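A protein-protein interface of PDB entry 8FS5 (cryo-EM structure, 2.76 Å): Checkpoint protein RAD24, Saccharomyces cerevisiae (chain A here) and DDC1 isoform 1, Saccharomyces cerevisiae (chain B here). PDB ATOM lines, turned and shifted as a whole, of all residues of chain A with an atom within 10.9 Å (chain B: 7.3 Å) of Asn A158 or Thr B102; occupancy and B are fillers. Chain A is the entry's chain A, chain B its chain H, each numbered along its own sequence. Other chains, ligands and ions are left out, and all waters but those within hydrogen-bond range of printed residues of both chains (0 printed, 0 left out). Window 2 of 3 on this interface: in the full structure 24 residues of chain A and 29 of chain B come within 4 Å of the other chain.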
ATOM      1  N   ASP A 154      -8.671 -35.812   4.301  1.00  0.00           N
ATOM      2  CA  ASP A 154      -7.410 -35.336   3.743  1.00  0.00           C
ATOM      3  C   ASP A 154      -7.598 -34.225   2.719  1.00  0.00           C
ATOM      4  O   ASP A 154      -6.612 -33.606   2.304  1.00  0.00           O
ATOM      5  CB  ASP A 154      -6.642 -36.501   3.112  1.00  0.00           C
ATOM      6  CG  ASP A 154      -6.315 -37.593   4.113  1.00  0.00           C
ATOM      7  OD1 ASP A 154      -6.910 -37.592   5.211  1.00  0.00           O
ATOM      8  OD2 ASP A 154      -5.462 -38.450   3.802  1.00  0.00           O
ATOM      9  N   CYS A 155      -8.834 -33.960   2.295  1.00  0.00           N
ATOM     10  CA  CYS A 155      -9.098 -32.912   1.317  1.00  0.00           C
ATOM     11  C   CYS A 155      -8.830 -31.532   1.907  1.00  0.00           C
ATOM     12  O   CYS A 155      -9.488 -31.123   2.869  1.00  0.00           O
ATOM     13  CB  CYS A 155     -10.539 -33.002   0.812  1.00  0.00           C
ATOM     14  SG  CYS A 155     -11.151 -31.495   0.024  1.00  0.00           S
ATOM     15  N   ILE A 156      -7.869 -30.812   1.339  1.00  0.00           N
ATOM     16  CA  ILE A 156      -7.494 -29.479   1.798  1.00  0.00           C
ATOM     17  C   ILE A 156      -7.794 -28.511   0.660  1.00  0.00           C
ATOM     18  O   ILE A 156      -7.006 -28.380  -0.284  1.00  0.00           O
ATOM     19  CB  ILE A 156      -6.024 -29.409   2.223  1.00  0.00           C
ATOM     20  CG1 ILE A 156      -5.712 -30.500   3.249  1.00  0.00           C
ATOM     21  CG2 ILE A 156      -5.697 -28.034   2.787  1.00  0.00           C
ATOM     22  CD1 ILE A 156      -4.242 -30.620   3.585  1.00  0.00           C
ATOM     23  N   VAL A 157      -8.932 -27.830   0.743  1.00  0.00           N
ATOM     24  CA  VAL A 157      -9.314 -26.845  -0.259  1.00  0.00           C
ATOM     25  C   VAL A 157      -8.709 -25.494   0.106  1.00  0.00           C
ATOM     26  O   VAL A 157      -8.257 -25.268   1.232  1.00  0.00           O
ATOM     27  CB  VAL A 157     -10.845 -26.756  -0.412  1.00  0.00           C
ATOM     28  CG1 VAL A 157     -11.362 -27.948  -1.198  1.00  0.00           C
ATOM     29  CG2 VAL A 157     -11.506 -26.700   0.946  1.00  0.00           C
ATOM     30  N   ASN A 158      -8.701 -24.584  -0.869  1.00  0.00           N
ATOM     31  CA  ASN A 158      -8.006 -23.305  -0.749  1.00  0.00           C
ATOM     32  C   ASN A 158      -8.550 -22.420   0.366  1.00  0.00           C
ATOM     33  O   ASN A 158      -7.832 -22.117   1.326  1.00  0.00           O
ATOM     34  CB  ASN A 158      -8.073 -22.551  -2.079  1.00  0.00           C
ATOM     35  CG  ASN A 158      -6.723 -22.028  -2.522  1.00  0.00           C
ATOM     36  OD1 ASN A 158      -5.740 -22.106  -1.785  1.00  0.00           O
ATOM     37  ND2 ASN A 158      -6.669 -21.488  -3.732  1.00  0.00           N
ATOM     38  N   ASP A 159      -9.806 -21.994   0.254  1.00  0.00           N
ATOM     39  CA  ASP A 159     -10.387 -21.042   1.201  1.00  0.00           C
ATOM     40  C   ASP A 159     -11.283 -21.802   2.172  1.00  0.00           C
ATOM     41  O   ASP A 159     -12.511 -21.751   2.075  1.00  0.00           O
ATOM     42  CB  ASP A 159     -11.155 -19.950   0.465  1.00  0.00           C
ATOM     43  CG  ASP A 159     -11.754 -18.920   1.404  1.00  0.00           C
ATOM     44  OD1 ASP A 159     -11.209 -18.729   2.511  1.00  0.00           O
ATOM     45  OD2 ASP A 159     -12.774 -18.301   1.033  1.00  0.00           O
ATOM     46  N   LEU A 160     -10.664 -22.515   3.110  1.00  0.00           N
ATOM     47  CA  LEU A 160     -11.396 -23.181   4.178  1.00  0.00           C
ATOM     48  C   LEU A 160     -10.459 -23.506   5.333  1.00  0.00           C
ATOM     49  O   LEU A 160      -9.420 -24.148   5.129  1.00  0.00           O
ATOM     50  CB  LEU A 160     -12.069 -24.458   3.674  1.00  0.00           C
ATOM     51  CG  LEU A 160     -13.169 -25.029   4.570  1.00  0.00           C
ATOM     52  CD1 LEU A 160     -14.205 -23.963   4.888  1.00  0.00           C
ATOM     53  CD2 LEU A 160     -13.819 -26.241   3.921  1.00  0.00           C
ATOM     54  N   PRO A 161     -10.781 -23.071   6.547  1.00  0.00           N
ATOM     55  CA  PRO A 161     -10.022 -23.518   7.716  1.00  0.00           C
ATOM     56  C   PRO A 161     -10.140 -25.027   7.891  1.00  0.00           C
ATOM     57  O   PRO A 161     -11.147 -25.635   7.521  1.00  0.00           O
ATOM     58  CB  PRO A 161     -10.679 -22.757   8.871  1.00  0.00           C
ATOM     59  CG  PRO A 161     -11.238 -21.532   8.231  1.00  0.00           C
ATOM     60  CD  PRO A 161     -11.727 -21.993   6.886  1.00  0.00           C
ATOM     61  N   GLN A 162      -9.087 -25.633   8.446  1.00  0.00           N
ATOM     62  CA  GLN A 162      -9.059 -27.083   8.611  1.00  0.00           C
ATOM     63  C   GLN A 162     -10.176 -27.558   9.533  1.00  0.00           C
ATOM     64  O   GLN A 162     -10.798 -28.599   9.292  1.00  0.00           O
ATOM     65  CB  GLN A 162      -7.695 -27.523   9.147  1.00  0.00           C
ATOM     66  CG  GLN A 162      -6.692 -27.891   8.067  1.00  0.00           C
ATOM     67  CD  GLN A 162      -7.020 -29.211   7.397  1.00  0.00           C
ATOM     68  OE1 GLN A 162      -6.824 -29.374   6.193  1.00  0.00           O
ATOM     69  NE2 GLN A 162      -7.524 -30.161   8.176  1.00  0.00           N
ATOM     70  N   MET A 163     -10.443 -26.804  10.601  1.00  0.00           N
ATOM     71  CA  MET A 163     -11.502 -27.175  11.530  1.00  0.00           C
ATOM     72  C   MET A 163     -12.889 -27.005  10.925  1.00  0.00           C
ATOM     73  O   MET A 163     -13.855 -27.570  11.448  1.00  0.00           O
ATOM     74  CB  MET A 163     -11.377 -26.344  12.809  1.00  0.00           C
ATOM     75  CG  MET A 163     -10.297 -26.846  13.748  1.00  0.00           C
ATOM     76  SD  MET A 163     -10.461 -26.246  15.437  1.00  0.00           S
ATOM     77  CE  MET A 163      -8.803 -25.627  15.720  1.00  0.00           C
ATOM     78  N   GLU A 164     -13.010 -26.244   9.833  1.00  0.00           N
ATOM     79  CA  GLU A 164     -14.288 -26.010   9.172  1.00  0.00           C
ATOM     80  C   GLU A 164     -14.543 -26.979   8.022  1.00  0.00           C
ATOM     81  O   GLU A 164     -15.567 -26.863   7.336  1.00  0.00           O
ATOM     82  CB  GLU A 164     -14.361 -24.567   8.671  1.00  0.00           C
ATOM     83  CG  GLU A 164     -15.635 -23.836   9.060  1.00  0.00           C
ATOM     84  CD  GLU A 164     -15.908 -23.896  10.549  1.00  0.00           C
ATOM     85  OE1 GLU A 164     -16.824 -24.638  10.960  1.00  0.00           O
ATOM     86  OE2 GLU A 164     -15.208 -23.196  11.311  1.00  0.00           O
ATOM     87  N   SER A 165     -13.637 -27.930   7.790  1.00  0.00           N
ATOM     88  CA  SER A 165     -13.790 -28.884   6.698  1.00  0.00           C
ATOM     89  C   SER A 165     -14.978 -29.816   6.904  1.00  0.00           C
ATOM     90  O   SER A 165     -15.719 -30.092   5.953  1.00  0.00           O
ATOM     91  CB  SER A 165     -12.510 -29.706   6.535  1.00  0.00           C
ATOM     92  OG  SER A 165     -11.898 -29.950   7.788  1.00  0.00           O
ATOM     93  N   GLU A 168     -18.561 -27.819   6.510  1.00  0.00           N
ATOM     94  CA  GLU A 168     -19.008 -27.658   5.133  1.00  0.00           C
ATOM     95  C   GLU A 168     -19.394 -28.978   4.482  1.00  0.00           C
ATOM     96  O   GLU A 168     -20.190 -28.975   3.536  1.00  0.00           O
ATOM     97  CB  GLU A 168     -17.926 -26.969   4.300  1.00  0.00           C
ATOM     98  CG  GLU A 168     -17.436 -25.661   4.892  1.00  0.00           C
ATOM     99  CD  GLU A 168     -18.522 -24.607   4.950  1.00  0.00           C
ATOM    100  OE1 GLU A 168     -19.339 -24.537   4.007  1.00  0.00           O
ATOM    101  OE2 GLU A 168     -18.562 -23.846   5.941  1.00  0.00           O
ATOM    102  N   PHE B  17      -6.899 -16.363 -13.281  1.00  0.00           N
ATOM    103  CA  PHE B  17      -6.447 -16.586 -11.912  1.00  0.00           C
ATOM    104  C   PHE B  17      -7.624 -16.721 -10.957  1.00  0.00           C
ATOM    105  O   PHE B  17      -7.628 -17.588 -10.077  1.00  0.00           O
ATOM    106  CB  PHE B  17      -5.525 -15.451 -11.467  1.00  0.00           C
ATOM    107  CG  PHE B  17      -5.315 -15.397  -9.980  1.00  0.00           C
ATOM    108  CD1 PHE B  17      -4.564 -16.365  -9.336  1.00  0.00           C
ATOM    109  CD2 PHE B  17      -5.874 -14.377  -9.226  1.00  0.00           C
ATOM    110  CE1 PHE B  17      -4.375 -16.319  -7.966  1.00  0.00           C
ATOM    111  CE2 PHE B  17      -5.686 -14.325  -7.857  1.00  0.00           C
ATOM    112  CZ  PHE B  17      -4.935 -15.297  -7.227  1.00  0.00           C
ATOM    113  N   ARG B  18      -8.638 -15.868 -11.113  1.00  0.00           N
ATOM    114  CA  ARG B  18      -9.780 -15.918 -10.207  1.00  0.00           C
ATOM    115  C   ARG B  18     -10.589 -17.195 -10.415  1.00  0.00           C
ATOM    116  O   ARG B  18     -11.058 -17.812  -9.450  1.00  0.00           O
ATOM    117  CB  ARG B  18     -10.647 -14.672 -10.394  1.00  0.00           C
ATOM    118  CG  ARG B  18     -11.967 -14.699  -9.644  1.00  0.00           C
ATOM    119  CD  ARG B  18     -11.785 -14.917  -8.147  1.00  0.00           C
ATOM    120  NE  ARG B  18     -10.807 -14.009  -7.563  1.00  0.00           N
ATOM    121  CZ  ARG B  18     -10.620 -13.850  -6.260  1.00  0.00           C
ATOM    122  NH1 ARG B  18     -11.334 -14.524  -5.373  1.00  0.00           N
ATOM    123  NH2 ARG B  18      -9.695 -12.994  -5.836  1.00  0.00           N
ATOM    124  N   ALA B  19     -10.751 -17.618 -11.673  1.00  0.00           N
ATOM    125  CA  ALA B  19     -11.460 -18.862 -11.955  1.00  0.00           C
ATOM    126  C   ALA B  19     -10.725 -20.059 -11.361  1.00  0.00           C
ATOM    127  O   ALA B  19     -11.340 -20.943 -10.750  1.00  0.00           O
ATOM    128  CB  ALA B  19     -11.643 -19.029 -13.464  1.00  0.00           C
ATOM    129  N   ILE B  20      -9.400 -20.100 -11.528  1.00  0.00           N
ATOM    130  CA  ILE B  20      -8.608 -21.173 -10.937  1.00  0.00           C
ATOM    131  C   ILE B  20      -8.679 -21.148  -9.417  1.00  0.00           C
ATOM    132  O   ILE B  20      -8.799 -22.207  -8.789  1.00  0.00           O
ATOM    133  CB  ILE B  20      -7.150 -21.095 -11.430  1.00  0.00           C
ATOM    134  CG1 ILE B  20      -7.080 -21.385 -12.931  1.00  0.00           C
ATOM    135  CG2 ILE B  20      -6.260 -22.064 -10.666  1.00  0.00           C
ATOM    136  CD1 ILE B  20      -7.568 -22.766 -13.309  1.00  0.00           C
ATOM    137  N   TYR B  21      -8.629 -19.964  -8.805  1.00  0.00           N
ATOM    138  CA  TYR B  21      -8.740 -19.853  -7.355  1.00  0.00           C
ATOM    139  C   TYR B  21     -10.081 -20.382  -6.859  1.00  0.00           C
ATOM    140  O   TYR B  21     -10.144 -21.107  -5.863  1.00  0.00           O
ATOM    141  CB  TYR B  21      -8.543 -18.395  -6.930  1.00  0.00           C
ATOM    142  CG  TYR B  21      -8.777 -18.141  -5.458  1.00  0.00           C
ATOM    143  CD1 TYR B  21      -7.842 -18.529  -4.509  1.00  0.00           C
ATOM    144  CD2 TYR B  21      -9.935 -17.511  -5.018  1.00  0.00           C
ATOM    145  CE1 TYR B  21      -8.052 -18.298  -3.162  1.00  0.00           C
ATOM    146  CE2 TYR B  21     -10.155 -17.277  -3.675  1.00  0.00           C
ATOM    147  CZ  TYR B  21      -9.211 -17.672  -2.751  1.00  0.00           C
ATOM    148  OH  TYR B  21      -9.424 -17.440  -1.412  1.00  0.00           O
ATOM    149  N   VAL B  22     -11.167 -20.033  -7.554  1.00  0.00           N
ATOM    150  CA  VAL B  22     -12.492 -20.502  -7.148  1.00  0.00           C
ATOM    151  C   VAL B  22     -12.599 -22.016  -7.297  1.00  0.00           C
ATOM    152  O   VAL B  22     -13.087 -22.715  -6.395  1.00  0.00           O
ATOM    153  CB  VAL B  22     -13.582 -19.770  -7.954  1.00  0.00           C
ATOM    154  CG1 VAL B  22     -14.926 -20.459  -7.783  1.00  0.00           C
ATOM    155  CG2 VAL B  22     -13.661 -18.320  -7.511  1.00  0.00           C
ATOM    156  N   LEU B  23     -12.134 -22.549  -8.429  1.00  0.00           N
ATOM    157  CA  LEU B  23     -12.160 -23.992  -8.636  1.00  0.00           C
ATOM    158  C   LEU B  23     -11.285 -24.737  -7.637  1.00  0.00           C
ATOM    159  O   LEU B  23     -11.575 -25.896  -7.322  1.00  0.00           O
ATOM    160  CB  LEU B  23     -11.726 -24.329 -10.064  1.00  0.00           C
ATOM    161  CG  LEU B  23     -12.674 -23.866 -11.175  1.00  0.00           C
ATOM    162  CD1 LEU B  23     -12.144 -24.268 -12.542  1.00  0.00           C
ATOM    163  CD2 LEU B  23     -14.085 -24.392 -10.961  1.00  0.00           C
ATOM    164  N   SER B  24     -10.228 -24.101  -7.135  1.00  0.00           N
ATOM    165  CA  SER B  24      -9.432 -24.659  -6.049  1.00  0.00           C
ATOM    166  C   SER B  24     -10.145 -24.594  -4.706  1.00  0.00           C
ATOM    167  O   SER B  24     -10.004 -25.524  -3.904  1.00  0.00           O
ATOM    168  CB  SER B  24      -8.090 -23.928  -5.953  1.00  0.00           C
ATOM    169  OG  SER B  24      -8.255 -22.628  -5.415  1.00  0.00           O
ATOM    170  N   THR B  25     -10.894 -23.524  -4.438  1.00  0.00           N
ATOM    171  CA  THR B  25     -11.713 -23.444  -3.235  1.00  0.00           C
ATOM    172  C   THR B  25     -12.835 -24.471  -3.217  1.00  0.00           C
ATOM    173  O   THR B  25     -13.246 -24.895  -2.132  1.00  0.00           O
ATOM    174  CB  THR B  25     -12.327 -22.045  -3.076  1.00  0.00           C
ATOM    175  OG1 THR B  25     -13.179 -21.761  -4.193  1.00  0.00           O
ATOM    176  CG2 THR B  25     -11.250 -20.983  -2.965  1.00  0.00           C
ATOM    177  N   ILE B  26     -13.336 -24.878  -4.380  1.00  0.00           N
ATOM    178  CA  ILE B  26     -14.402 -25.874  -4.412  1.00  0.00           C
ATOM    179  C   ILE B  26     -13.879 -27.291  -4.169  1.00  0.00           C
ATOM    180  O   ILE B  26     -14.452 -28.029  -3.361  1.00  0.00           O
ATOM    181  CB  ILE B  26     -15.168 -25.784  -5.740  1.00  0.00           C
ATOM    182  CG1 ILE B  26     -15.837 -24.415  -5.858  1.00  0.00           C
ATOM    183  CG2 ILE B  26     -16.200 -26.898  -5.845  1.00  0.00           C
ATOM    184  CD1 ILE B  26     -16.640 -24.236  -7.112  1.00  0.00           C
ATOM    185  N   GLN B  27     -12.799 -27.686  -4.839  1.00  0.00           N
ATOM    186  CA  GLN B  27     -12.230 -29.015  -4.651  1.00  0.00           C
ATOM    187  C   GLN B  27     -10.713 -28.890  -4.687  1.00  0.00           C
ATOM    188  O   GLN B  27     -10.163 -27.990  -5.328  1.00  0.00           O
ATOM    189  CB  GLN B  27     -12.741 -29.995  -5.716  1.00  0.00           C
ATOM    190  CG  GLN B  27     -12.218 -31.423  -5.612  1.00  0.00           C
ATOM    191  CD  GLN B  27     -12.925 -32.228  -4.538  1.00  0.00           C
ATOM    192  OE1 GLN B  27     -12.686 -32.039  -3.346  1.00  0.00           O
ATOM    193  NE2 GLN B  27     -13.800 -33.133  -4.959  1.00  0.00           N
ATOM    194  N   ASP B  28     -10.045 -29.807  -3.980  1.00  0.00           N
ATOM    195  CA  ASP B  28      -8.591 -29.744  -3.855  1.00  0.00           C
ATOM    196  C   ASP B  28      -7.900 -29.900  -5.206  1.00  0.00           C
ATOM    197  O   ASP B  28      -6.879 -29.251  -5.463  1.00  0.00           O
ATOM    198  CB  ASP B  28      -8.104 -30.810  -2.871  1.00  0.00           C
ATOM    199  CG  ASP B  28      -8.459 -32.219  -3.311  1.00  0.00           C
ATOM    200  OD1 ASP B  28      -9.416 -32.378  -4.096  1.00  0.00           O
ATOM    201  OD2 ASP B  28      -7.781 -33.169  -2.866  1.00  0.00           O
ATOM    202  N   ILE B  30      -8.273 -29.477  -9.243  1.00  0.00           N
ATOM    203  CA  ILE B  30      -9.060 -28.896 -10.323  1.00  0.00           C
ATOM    204  C   ILE B  30      -9.032 -29.819 -11.536  1.00  0.00           C
ATOM    205  O   ILE B  30      -7.999 -30.410 -11.878  1.00  0.00           O
ATOM    206  CB  ILE B  30      -8.543 -27.490 -10.679  1.00  0.00           C
ATOM    207  CG1 ILE B  30      -8.586 -26.582  -9.452  1.00  0.00           C
ATOM    208  CG2 ILE B  30      -9.360 -26.869 -11.803  1.00  0.00           C
ATOM    209  CD1 ILE B  30      -8.059 -25.195  -9.715  1.00  0.00           C
ATOM    210  N   ASN B  97      -3.566 -30.277  -8.972  1.00  0.00           N
ATOM    211  CA  ASN B  97      -3.835 -29.721  -7.651  1.00  0.00           C
ATOM    212  C   ASN B  97      -4.222 -28.251  -7.761  1.00  0.00           C
ATOM    213  O   ASN B  97      -3.523 -27.456  -8.396  1.00  0.00           O
ATOM    214  CB  ASN B  97      -2.607 -29.882  -6.755  1.00  0.00           C
ATOM    215  CG  ASN B  97      -2.921 -29.667  -5.285  1.00  0.00           C
ATOM    216  OD1 ASN B  97      -4.033 -29.285  -4.921  1.00  0.00           O
ATOM    217  ND2 ASN B  97      -1.934 -29.909  -4.429  1.00  0.00           N
ATOM    218  N   GLY B  98      -5.344 -27.895  -7.142  1.00  0.00           N
ATOM    219  CA  GLY B  98      -5.832 -26.532  -7.177  1.00  0.00           C
ATOM    220  C   GLY B  98      -4.966 -25.537  -6.435  1.00  0.00           C
ATOM    221  O   GLY B  98      -4.694 -24.441  -6.937  1.00  0.00           O
ATOM    222  N   ARG B  99      -4.527 -25.912  -5.230  1.00  0.00           N
ATOM    223  CA  ARG B  99      -3.677 -25.034  -4.437  1.00  0.00           C
ATOM    224  C   ARG B  99      -2.316 -24.820  -5.080  1.00  0.00           C
ATOM    225  O   ARG B  99      -1.659 -23.813  -4.795  1.00  0.00           O
ATOM    226  CB  ARG B  99      -3.505 -25.602  -3.028  1.00  0.00           C
ATOM    227  CG  ARG B  99      -4.565 -25.141  -2.040  1.00  0.00           C
ATOM    228  CD  ARG B  99      -4.437 -25.779  -0.651  1.00  0.00           C
ATOM    229  NE  ARG B  99      -4.177 -27.215  -0.669  1.00  0.00           N
ATOM    230  CZ  ARG B  99      -2.973 -27.769  -0.594  1.00  0.00           C
ATOM    231  NH1 ARG B  99      -1.880 -27.032  -0.482  1.00  0.00           N
ATOM    232  NH2 ARG B  99      -2.865 -29.093  -0.631  1.00  0.00           N
ATOM    233  N   HIS B 100      -1.877 -25.744  -5.933  1.00  0.00           N
ATOM    234  CA  HIS B 100      -0.621 -25.596  -6.654  1.00  0.00           C
ATOM    235  C   HIS B 100      -0.769 -24.725  -7.895  1.00  0.00           C
ATOM    236  O   HIS B 100       0.112 -23.910  -8.189  1.00  0.00           O
ATOM    237  CB  HIS B 100      -0.077 -26.972  -7.039  1.00  0.00           C
ATOM    238  CG  HIS B 100       0.423 -27.771  -5.876  1.00  0.00           C
ATOM    239  ND1 HIS B 100       0.971 -29.027  -6.016  1.00  0.00           N
ATOM    240  CD2 HIS B 100       0.459 -27.490  -4.552  1.00  0.00           C
ATOM    241  CE1 HIS B 100       1.323 -29.486  -4.829  1.00  0.00           C
ATOM    242  NE2 HIS B 100       1.022 -28.572  -3.923  1.00  0.00           N
ATOM    243  N   LEU B 101      -1.870 -24.880  -8.633  1.00  0.00           N
ATOM    244  CA  LEU B 101      -2.105 -24.068  -9.819  1.00  0.00           C
ATOM    245  C   LEU B 101      -2.523 -22.643  -9.480  1.00  0.00           C
ATOM    246  O   LEU B 101      -2.305 -21.738 -10.294  1.00  0.00           O
ATOM    247  CB  LEU B 101      -3.168 -24.725 -10.702  1.00  0.00           C
ATOM    248  CG  LEU B 101      -3.318 -24.198 -12.132  1.00  0.00           C
ATOM    249  CD1 LEU B 101      -2.019 -24.363 -12.906  1.00  0.00           C
ATOM    250  CD2 LEU B 101      -4.462 -24.900 -12.847  1.00  0.00           C
ATOM    251  N   THR B 102      -3.102 -22.417  -8.301  1.00  0.00           N
ATOM    252  CA  THR B 102      -3.528 -21.081  -7.904  1.00  0.00           C
ATOM    253  C   THR B 102      -2.363 -20.181  -7.505  1.00  0.00           C
ATOM    254  O   THR B 102      -2.551 -18.964  -7.400  1.00  0.00           O
ATOM    255  CB  THR B 102      -4.535 -21.166  -6.752  1.00  0.00           C
ATOM    256  OG1 THR B 102      -5.282 -19.945  -6.679  1.00  0.00           O
ATOM    257  CG2 THR B 102      -3.821 -21.396  -5.430  1.00  0.00           C
ATOM    258  N   THR B 103      -1.177 -20.740  -7.283  1.00  0.00           N
ATOM    259  CA  THR B 103       0.015 -19.951  -7.000  1.00  0.00           C
ATOM    260  C   THR B 103       0.852 -19.683  -8.238  1.00  0.00           C
ATOM    261  O   THR B 103       1.525 -18.651  -8.309  1.00  0.00           O
ATOM    262  CB  THR B 103       0.884 -20.646  -5.940  1.00  0.00           C
ATOM    263  OG1 THR B 103       1.497 -21.810  -6.507  1.00  0.00           O
ATOM    264  CG2 THR B 103       0.043 -21.048  -4.739  1.00  0.00           C
ATOM    265  N   ILE B 104       0.836 -20.593  -9.216  1.00  0.00           N
ATOM    266  CA  ILE B 104       1.480 -20.324 -10.495  1.00  0.00           C
ATOM    267  C   ILE B 104       0.787 -19.190 -11.229  1.00  0.00           C
ATOM    268  O   ILE B 104       1.451 -18.285 -11.745  1.00  0.00           O
ATOM    269  CB  ILE B 104       1.504 -21.592 -11.371  1.00  0.00           C
ATOM    270  CG1 ILE B 104       2.185 -22.749 -10.642  1.00  0.00           C
ATOM    271  CG2 ILE B 104       2.218 -21.317 -12.677  1.00  0.00           C
ATOM    272  CD1 ILE B 104       2.203 -24.026 -11.451  1.00  0.00           C
ATOM    273  N   SER B 105      -0.545 -19.209 -11.278  1.00  0.00           N
ATOM    274  CA  SER B 105      -1.313 -18.175 -11.956  1.00  0.00           C
ATOM    275  C   SER B 105      -1.477 -16.911 -11.127  1.00  0.00           C
ATOM    276  O   SER B 105      -2.035 -15.929 -11.630  1.00  0.00           O
ATOM    277  CB  SER B 105      -2.699 -18.707 -12.339  1.00  0.00           C
ATOM    278  OG  SER B 105      -3.472 -18.993 -11.186  1.00  0.00           O
ATOM    279  N   ARG B 106      -1.019 -16.916  -9.876  1.00  0.00           N
ATOM    280  CA  ARG B 106      -1.058 -15.718  -9.049  1.00  0.00           C
ATOM    281  C   ARG B 106      -0.218 -14.614  -9.675  1.00  0.00           C
ATOM    282  O   ARG B 106       0.914 -14.847 -10.105  1.00  0.00           O
ATOM    283  CB  ARG B 106      -0.551 -16.035  -7.641  1.00  0.00           C
ATOM    284  CG  ARG B 106      -0.658 -14.873  -6.665  1.00  0.00           C
ATOM    285  CD  ARG B 106      -0.716 -15.358  -5.225  1.00  0.00           C
ATOM    286  NE  ARG B 106      -2.051 -15.230  -4.654  1.00  0.00           N
ATOM    287  CZ  ARG B 106      -2.904 -16.235  -4.512  1.00  0.00           C
ATOM    288  NH1 ARG B 106      -2.593 -17.465  -4.888  1.00  0.00           N
ATOM    289  NH2 ARG B 106      -4.099 -16.002  -3.976  1.00  0.00           N
ATOM    290  N   LYS B 107      -0.781 -13.416  -9.728  1.00  0.00           N
ATOM    291  CA  LYS B 107      -0.064 -12.280 -10.290  1.00  0.00           C
ATOM    292  C   LYS B 107       0.877 -11.706  -9.239  1.00  0.00           C
ATOM    293  O   LYS B 107       0.409 -11.226  -8.198  1.00  0.00           O
ATOM    294  CB  LYS B 107      -1.047 -11.217 -10.769  1.00  0.00           C
ATOM    295  CG  LYS B 107      -0.392  -9.945 -11.281  1.00  0.00           C
ATOM    296  CD  LYS B 107      -0.909  -8.723 -10.541  1.00  0.00           C
ATOM    297  CE  LYS B 107      -0.057  -7.499 -10.834  1.00  0.00           C
ATOM    298  NZ  LYS B 107      -0.438  -6.340  -9.980  1.00  0.00           N
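SG of Cys A155 is in hydrogen-bond range of OE1 of Gln B27 (3.7 Å).
O of Ile A156 sits at hydrogen-bond distance from NE of Arg B99.
The side-chain hydroxyl of Ser B24 lies within hydrogen-bond range of the side-chain amide nitrogen of Asn A158 (2.6 Å).
O of Val B22 is in hydrogen-bond range of OG1 of Thr B25 (2.4 Å).
The side-chain carboxylate of Asp B28 lies close to the side-chain amide oxygen of Gln B27.
O of Asp B28 lies close to OD1 of Asn B97.
N of Gly B98 lies within hydrogen-bond range of O of Asp B28.
The side-chain amide oxygen (OD1) of Asn B97 sits at hydrogen-bond distance from the backbone NH (N) of Arg B99 (3.4 Å).
The backbone carbonyl oxygen (O) of Thr B102 lies within hydrogen-bond range of the guanidinium group (NH1) of Arg B106.
Ile A156 touches Asp B28.
Ser B24 touches Val A157 (O to CB, 3.8 Å).
Val A157 touches Thr B25 (CB to O, 3.5 Å).
Ile B26 touches Val A157 (O to CG1, 3.8 Å).
N of Asp B28 touches CG1 of Val A157, 3.6 Å away.
Thr B25 touches Asn A158 (CG2 to CB, 3.7 Å).
Arg B99 touches Asn A158 (CG to OD1, 3.3 Å).
Asn A158 touches Thr B102 (ND2 to CG2, 3.3 Å).
CB of Asp A159 touches OH of Tyr B21, at 3.6 Å.
CG2 of Thr B25 touches CB of Asp A159, 3.6 Å away.
Of chain B, only Tyr B21 (3.3 Å), Ser B24 (2.6 Å), Thr B25 (3.7 Å), Arg B99 (3.3 Å) and Thr B102 (3.3 Å) come within 4 Å of Asn A158.
Of the printed residues of chain A, Thr B102 touches Asn A158 (3.3 Å).
Ser B24 touches two residues of chain A.
No residue of chain A comes within 4 Å of Gly B98.
No residue of chain A comes within 4 Å of Leu B101.
No residue of chain A comes within 4 Å of Thr B103.
No residue of chain A comes within 4 Å of Ser B105.
Arg B106 touches none of the printed residues of chain A.
Of the printed residues of chain B, Val A157 touches Ser B24 (3.8 Å), Thr B25 (3.5 Å), Ile B26 (3.8 Å), Gln B27 (3.7 Å) and Asp B28 (3.6 Å).
Of the printed residues of chain B, Cys A155 touches Gln B27.
Of the printed residues of chain B, Ile A156 touches Asp B28 (3.7 Å) and Arg B99 (3.1 Å).
Of the printed residues of chain A, Ile B26 touches Val A157.
Gln A162 touches none of the printed residues of chain B.
The nearest residue of chain B that does not touch Asn A158 is Gly B98 (4.8 Å).
The nearest residue of chain A that does not touch Thr B102 is Asp A159 (8.3 Å).
Hydrophobic or aromatic side chains of chain A that line the printed part of chain B: Ile A156 and Val A157.
Of the 24 printed residues of chain B, 8 touch a printed residue of chain A.
Hydrophobic or aromatic side chains of chain B that line the printed part of chain A: Tyr B21.
Among the printed residues, 15 pairs touch across the chains.
Among the printed residues, no Asp or Glu carboxylate lies within 4 Å of a Lys or Arg side-chain nitrogen of the other chain.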
